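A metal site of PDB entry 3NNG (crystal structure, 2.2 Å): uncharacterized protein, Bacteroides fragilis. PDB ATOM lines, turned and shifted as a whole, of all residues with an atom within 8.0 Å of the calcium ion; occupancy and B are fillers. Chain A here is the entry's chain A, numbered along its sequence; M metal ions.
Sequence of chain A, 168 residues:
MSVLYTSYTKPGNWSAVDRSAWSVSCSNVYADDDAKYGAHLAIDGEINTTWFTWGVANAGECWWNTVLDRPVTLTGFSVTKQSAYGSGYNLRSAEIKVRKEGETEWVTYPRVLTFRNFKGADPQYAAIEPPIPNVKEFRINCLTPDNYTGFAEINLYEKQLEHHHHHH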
ATOM      1  N   ARG A  19      22.133   8.819  12.927  1.00  0.00           N
ATOM      2  CA  ARG A  19      22.216   9.159  11.497  1.00  0.00           C
ATOM      3  C   ARG A  19      23.208   8.287  10.705  1.00  0.00           C
ATOM      4  O   ARG A  19      23.279   8.370   9.478  1.00  0.00           O
ATOM      5  CB  ARG A  19      22.586  10.645  11.330  1.00  0.00           C
ATOM      6  CG  ARG A  19      21.576  11.629  11.946  1.00  0.00           C
ATOM      7  CD  ARG A  19      22.110  13.053  12.014  1.00  0.00           C
ATOM      8  NE  ARG A  19      23.270  13.156  12.894  1.00  0.00           N
ATOM      9  CZ  ARG A  19      23.936  14.281  13.155  1.00  0.00           C
ATOM     10  NH1 ARG A  19      23.569  15.442  12.595  1.00  0.00           N
ATOM     11  NH2 ARG A  19      24.992  14.249  13.966  1.00  0.00           N
ATOM     12  N   GLY A  38      29.941  18.536   0.788  1.00  0.00           N
ATOM     13  CA  GLY A  38      28.955  17.515   0.462  1.00  0.00           C
ATOM     14  C   GLY A  38      27.840  17.287   1.485  1.00  0.00           C
ATOM     15  O   GLY A  38      27.944  17.670   2.652  1.00  0.00           O
ATOM     16  N   ALA A  39      26.773  16.621   1.041  1.00  0.00           N
ATOM     17  CA  ALA A  39      25.580  16.435   1.864  1.00  0.00           C
ATOM     18  C   ALA A  39      25.869  15.759   3.199  1.00  0.00           C
ATOM     19  O   ALA A  39      25.245  16.103   4.221  1.00  0.00           O
ATOM     20  CB  ALA A  39      24.537  15.651   1.083  1.00  0.00           C
ATOM     21  N   HIS A  40      26.801  14.803   3.191  1.00  0.00           N
ATOM     22  CA  HIS A  40      27.091  13.972   4.352  1.00  0.00           C
ATOM     23  C   HIS A  40      27.719  14.806   5.464  1.00  0.00           C
ATOM     24  O   HIS A  40      27.660  14.451   6.635  1.00  0.00           O
ATOM     25  CB  HIS A  40      28.042  12.831   3.954  1.00  0.00           C
ATOM     26  CG  HIS A  40      29.371  13.298   3.465  1.00  0.00           C
ATOM     27  ND1 HIS A  40      29.583  13.720   2.161  1.00  0.00           N
ATOM     28  CD2 HIS A  40      30.570  13.433   4.080  1.00  0.00           C
ATOM     29  CE1 HIS A  40      30.837  14.078   2.005  1.00  0.00           C
ATOM     30  NE2 HIS A  40      31.460  13.925   3.157  1.00  0.00           N
ATOM     31  N   LEU A  41      28.327  15.930   5.088  1.00  0.00           N
ATOM     32  CA  LEU A  41      28.911  16.807   6.102  1.00  0.00           C
ATOM     33  C   LEU A  41      27.861  17.456   6.990  1.00  0.00           C
ATOM     34  O   LEU A  41      28.182  17.923   8.064  1.00  0.00           O
ATOM     35  CB  LEU A  41      29.806  17.882   5.461  1.00  0.00           C
ATOM     36  CG  LEU A  41      31.017  17.357   4.685  1.00  0.00           C
ATOM     37  CD1 LEU A  41      31.785  18.499   4.031  1.00  0.00           C
ATOM     38  CD2 LEU A  41      31.954  16.542   5.577  1.00  0.00           C
ATOM     39  N   ALA A  42      26.597  17.474   6.556  1.00  0.00           N
ATOM     40  CA  ALA A  42      25.532  17.989   7.429  1.00  0.00           C
ATOM     41  C   ALA A  42      25.132  17.027   8.570  1.00  0.00           C
ATOM     42  O   ALA A  42      24.395  17.422   9.481  1.00  0.00           O
ATOM     43  CB  ALA A  42      24.299  18.353   6.611  1.00  0.00           C
ATOM     44  N   ILE A  43      25.581  15.774   8.509  1.00  0.00           N
ATOM     45  CA  ILE A  43      25.185  14.797   9.521  1.00  0.00           C
ATOM     46  C   ILE A  43      26.365  14.086  10.188  1.00  0.00           C
ATOM     47  O   ILE A  43      26.237  12.948  10.625  1.00  0.00           O
ATOM     48  CB  ILE A  43      24.215  13.733   8.948  1.00  0.00           C
ATOM     49  CG1 ILE A  43      24.855  12.992   7.773  1.00  0.00           C
ATOM     50  CG2 ILE A  43      22.879  14.387   8.503  1.00  0.00           C
ATOM     51  CD1 ILE A  43      24.290  11.599   7.538  1.00  0.00           C
ATOM     52  N   ASP A  44      27.510  14.753  10.272  1.00  0.00           N
ATOM     53  CA  ASP A  44      28.714  14.095  10.813  1.00  0.00           C
ATOM     54  C   ASP A  44      29.025  14.471  12.261  1.00  0.00           C
ATOM     55  O   ASP A  44      30.009  14.004  12.830  1.00  0.00           O
ATOM     56  CB  ASP A  44      29.933  14.316   9.905  1.00  0.00           C
ATOM     57  CG  ASP A  44      30.343  15.781   9.832  1.00  0.00           C
ATOM     58  OD1 ASP A  44      29.792  16.589  10.609  1.00  0.00           O
ATOM     59  OD2 ASP A  44      31.240  16.105   9.021  1.00  0.00           O
ATOM     60  N   GLY A  45      28.183  15.310  12.861  1.00  0.00           N
ATOM     61  CA  GLY A  45      28.331  15.685  14.253  1.00  0.00           C
ATOM     62  C   GLY A  45      29.251  16.863  14.507  1.00  0.00           C
ATOM     63  O   GLY A  45      29.474  17.222  15.671  1.00  0.00           O
ATOM     64  N   GLU A  46      29.788  17.471  13.445  1.00  0.00           N
ATOM     65  CA  GLU A  46      30.802  18.504  13.580  1.00  0.00           C
ATOM     66  C   GLU A  46      30.324  19.881  13.080  1.00  0.00           C
ATOM     67  O   GLU A  46      29.891  20.014  11.948  1.00  0.00           O
ATOM     68  CB  GLU A  46      32.055  18.093  12.802  1.00  0.00           C
ATOM     69  CG  GLU A  46      33.107  19.189  12.658  1.00  0.00           C
ATOM     70  CD  GLU A  46      33.625  19.652  14.003  1.00  0.00           C
ATOM     71  OE1 GLU A  46      33.612  20.877  14.265  1.00  0.00           O
ATOM     72  OE2 GLU A  46      34.048  18.794  14.800  1.00  0.00           O
ATOM     73  N   ILE A  47      30.412  20.911  13.915  1.00  0.00           N
ATOM     74  CA  ILE A  47      29.900  22.224  13.512  1.00  0.00           C
ATOM     75  C   ILE A  47      30.737  22.856  12.399  1.00  0.00           C
ATOM     76  O   ILE A  47      30.246  23.646  11.577  1.00  0.00           O
ATOM     77  CB  ILE A  47      29.751  23.205  14.707  1.00  0.00           C
ATOM     78  CG1 ILE A  47      28.985  24.464  14.291  1.00  0.00           C
ATOM     79  CG2 ILE A  47      31.129  23.543  15.345  1.00  0.00           C
ATOM     80  CD1 ILE A  47      27.466  24.290  14.203  1.00  0.00           C
ATOM     81  N   ASN A  48      32.007  22.466  12.335  1.00  0.00           N
ATOM     82  CA  ASN A  48      32.939  23.113  11.415  1.00  0.00           C
ATOM     83  C   ASN A  48      33.003  22.491  10.031  1.00  0.00           C
ATOM     84  O   ASN A  48      33.762  22.944   9.179  1.00  0.00           O
ATOM     85  CB  ASN A  48      34.324  23.207  12.032  1.00  0.00           C
ATOM     86  CG  ASN A  48      34.420  24.347  13.035  1.00  0.00           C
ATOM     87  OD1 ASN A  48      34.139  25.497  12.692  1.00  0.00           O
ATOM     88  ND2 ASN A  48      34.795  24.033  14.268  1.00  0.00           N
ATOM     89  N   THR A  49      32.205  21.458   9.794  1.00  0.00           N
ATOM     90  CA  THR A  49      32.056  20.942   8.440  1.00  0.00           C
ATOM     91  C   THR A  49      30.616  21.190   8.031  1.00  0.00           C
ATOM     92  O   THR A  49      29.702  21.069   8.837  1.00  0.00           O
ATOM     93  CB  THR A  49      32.376  19.441   8.364  1.00  0.00           C
ATOM     94  OG1 THR A  49      31.474  18.737   9.222  1.00  0.00           O
ATOM     95  CG2 THR A  49      33.828  19.174   8.826  1.00  0.00           C
ATOM     96  N   THR A  50      30.388  21.544   6.779  1.00  0.00           N
ATOM     97  CA  THR A  50      29.046  21.939   6.426  1.00  0.00           C
ATOM     98  C   THR A  50      28.682  21.529   5.011  1.00  0.00           C
ATOM     99  O   THR A  50      29.543  21.437   4.128  1.00  0.00           O
ATOM    100  CB  THR A  50      28.888  23.472   6.555  1.00  0.00           C
ATOM    101  OG1 THR A  50      27.535  23.846   6.275  1.00  0.00           O
ATOM    102  CG2 THR A  50      29.823  24.154   5.580  1.00  0.00           C
ATOM    103  N   TRP A  51      27.394  21.257   4.823  1.00  0.00           N
ATOM    104  CA  TRP A  51      26.813  21.211   3.485  1.00  0.00           C
ATOM    105  C   TRP A  51      26.634  22.663   3.018  1.00  0.00           C
ATOM    106  O   TRP A  51      26.214  23.526   3.783  1.00  0.00           O
ATOM    107  CB  TRP A  51      25.458  20.489   3.500  1.00  0.00           C
ATOM    108  CG  TRP A  51      24.738  20.589   2.190  1.00  0.00           C
ATOM    109  CD1 TRP A  51      25.185  20.120   0.994  1.00  0.00           C
ATOM    110  CD2 TRP A  51      23.461  21.207   1.943  1.00  0.00           C
ATOM    111  NE1 TRP A  51      24.259  20.388   0.008  1.00  0.00           N
ATOM    112  CE2 TRP A  51      23.199  21.065   0.559  1.00  0.00           C
ATOM    113  CE3 TRP A  51      22.520  21.858   2.755  1.00  0.00           C
ATOM    114  CZ2 TRP A  51      22.025  21.552  -0.030  1.00  0.00           C
ATOM    115  CZ3 TRP A  51      21.368  22.350   2.166  1.00  0.00           C
ATOM    116  CH2 TRP A  51      21.123  22.192   0.784  1.00  0.00           C
ATOM    117  N   THR A  80      21.651  24.065  12.089  1.00  0.00           N
ATOM    118  CA  THR A  80      22.590  25.052  12.640  1.00  0.00           C
ATOM    119  C   THR A  80      22.958  26.061  11.563  1.00  0.00           C
ATOM    120  O   THR A  80      22.476  25.977  10.425  1.00  0.00           O
ATOM    121  CB  THR A  80      23.888  24.381  13.126  1.00  0.00           C
ATOM    122  OG1 THR A  80      24.527  23.731  12.020  1.00  0.00           O
ATOM    123  CG2 THR A  80      23.589  23.323  14.221  1.00  0.00           C
ATOM    124  N   LYS A  81      23.813  27.027  11.901  1.00  0.00           N
ATOM    125  CA  LYS A  81      24.479  27.810  10.873  1.00  0.00           C
ATOM    126  C   LYS A  81      25.176  26.875   9.886  1.00  0.00           C
ATOM    127  O   LYS A  81      25.444  25.704  10.201  1.00  0.00           O
ATOM    128  CB  LYS A  81      25.537  28.720  11.509  1.00  0.00           C
ATOM    129  CG  LYS A  81      26.627  27.927  12.243  1.00  0.00           C
ATOM    130  CD  LYS A  81      27.791  28.849  12.599  1.00  0.00           C
ATOM    131  CE  LYS A  81      28.882  28.098  13.338  1.00  0.00           C
ATOM    132  NZ  LYS A  81      30.037  28.978  13.668  1.00  0.00           N
ATOM    133  N   SER A  83      28.930  26.735   8.073  1.00  0.00           N
ATOM    134  CA  SER A  83      30.219  27.265   8.522  1.00  0.00           C
ATOM    135  C   SER A  83      31.215  27.411   7.393  1.00  0.00           C
ATOM    136  O   SER A  83      32.421  27.354   7.618  1.00  0.00           O
ATOM    137  CB  SER A  83      30.810  26.384   9.630  1.00  0.00           C
ATOM    138  OG  SER A  83      30.928  25.035   9.175  1.00  0.00           O
ATOM    139  N   PHE A 151      23.925  24.183   5.721  1.00  0.00           N
ATOM    140  CA  PHE A 151      23.919  24.054   7.168  1.00  0.00           C
ATOM    141  C   PHE A 151      24.926  23.003   7.628  1.00  0.00           C
ATOM    142  O   PHE A 151      25.235  22.080   6.886  1.00  0.00           O
ATOM    143  CB  PHE A 151      22.518  23.761   7.724  1.00  0.00           C
ATOM    144  CG  PHE A 151      21.731  22.737   6.942  1.00  0.00           C
ATOM    145  CD1 PHE A 151      20.582  23.101   6.248  1.00  0.00           C
ATOM    146  CD2 PHE A 151      22.123  21.400   6.919  1.00  0.00           C
ATOM    147  CE1 PHE A 151      19.855  22.161   5.528  1.00  0.00           C
ATOM    148  CE2 PHE A 151      21.392  20.453   6.220  1.00  0.00           C
ATOM    149  CZ  PHE A 151      20.259  20.831   5.505  1.00  0.00           C
ATOM    150  N   ALA A 152      25.461  23.183   8.827  1.00  0.00           N
ATOM    151  CA  ALA A 152      26.587  22.369   9.273  1.00  0.00           C
ATOM    152  C   ALA A 152      26.088  21.109   9.922  1.00  0.00           C
ATOM    153  O   ALA A 152      26.733  20.069   9.832  1.00  0.00           O
ATOM    154  CB  ALA A 152      27.461  23.147  10.220  1.00  0.00           C
ATOM    155  N   GLU A 153      24.929  21.185  10.553  1.00  0.00           N
ATOM    156  CA  GLU A 153      24.367  20.040  11.226  1.00  0.00           C
ATOM    157  C   GLU A 153      22.856  20.083  11.142  1.00  0.00           C
ATOM    158  O   GLU A 153      22.239  21.075  11.521  1.00  0.00           O
ATOM    159  CB  GLU A 153      24.783  20.054  12.702  1.00  0.00           C
ATOM    160  CG  GLU A 153      26.200  19.547  12.890  1.00  0.00           C
ATOM    161  CD  GLU A 153      26.316  18.088  12.478  1.00  0.00           C
ATOM    162  OE1 GLU A 153      25.539  17.259  13.004  1.00  0.00           O
ATOM    163  OE2 GLU A 153      27.162  17.763  11.624  1.00  0.00           O
ATOM    164  N   ILE A 154      22.275  19.009  10.626  1.00  0.00           N
ATOM    165  CA  ILE A 154      20.831  18.810  10.695  1.00  0.00           C
ATOM    166  C   ILE A 154      20.526  17.530  11.465  1.00  0.00           C
ATOM    167  O   ILE A 154      21.257  16.537  11.363  1.00  0.00           O
ATOM    168  CB  ILE A 154      20.207  18.708   9.312  1.00  0.00           C
ATOM    169  CG1 ILE A 154      18.683  18.686   9.447  1.00  0.00           C
ATOM    170  CG2 ILE A 154      20.738  17.459   8.558  1.00  0.00           C
ATOM    171  CD1 ILE A 154      17.957  18.913   8.131  1.00  0.00           C
HETATM  172 CA    CA M   1      28.915  18.993  10.059  1.00  0.00          CA
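OE1 of Glu 46 is in hydrogen-bond range of N of Asn 48, 3.0 Å away.
The backbone NH of Ala 152 is in hydrogen-bond range of the side-chain hydroxyl of Thr 50 (3.4 Å).
The backbone NH (N) of Ala 152 lies within hydrogen-bond range of the side-chain hydroxyl (OG1) of Thr 80 (3.4 Å).
The backbone NH (N) of Ala 152 is in hydrogen-bond range of the backbone carbonyl oxygen (O) of Lys 81 (2.9 Å).
The side-chain carboxylate (OE1) of Glu 153 sits at hydrogen-bond distance from the backbone NH (N) of Gly 45.
The side-chain hydroxyl (OG1) of Thr 80 sits at hydrogen-bond distance from the backbone NH (N) of Glu 153 (3.0 Å).
The guanidinium group (NH1) of Arg 19 lies within salt-bridge range of the side-chain carboxylate (OE1) of Glu 153, 2.7 Å away.
Within 4 Å of the calcium ion: Leu 41, Asp 44, Glu 46, Thr 49, Ala 152 and Glu 153.
The calcium ion is bound by O of Glu 46 (2.4 Å).
O of Leu 41 binds the calcium ion (2.4 Å).
The backbone carbonyl oxygen (O) of Ala 152 binds the calcium ion (2.4 Å).
O of Thr 49 is bound to the calcium ion, 2.5 Å away.
OD1 of Asp 44 binds the calcium ion (2.6 Å).
OE2 of Glu 153 binds the calcium ion (2.7 Å).
OG1 of Thr 49 binds the calcium ion.
The calcium ion has seven donor atoms within binding distance.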
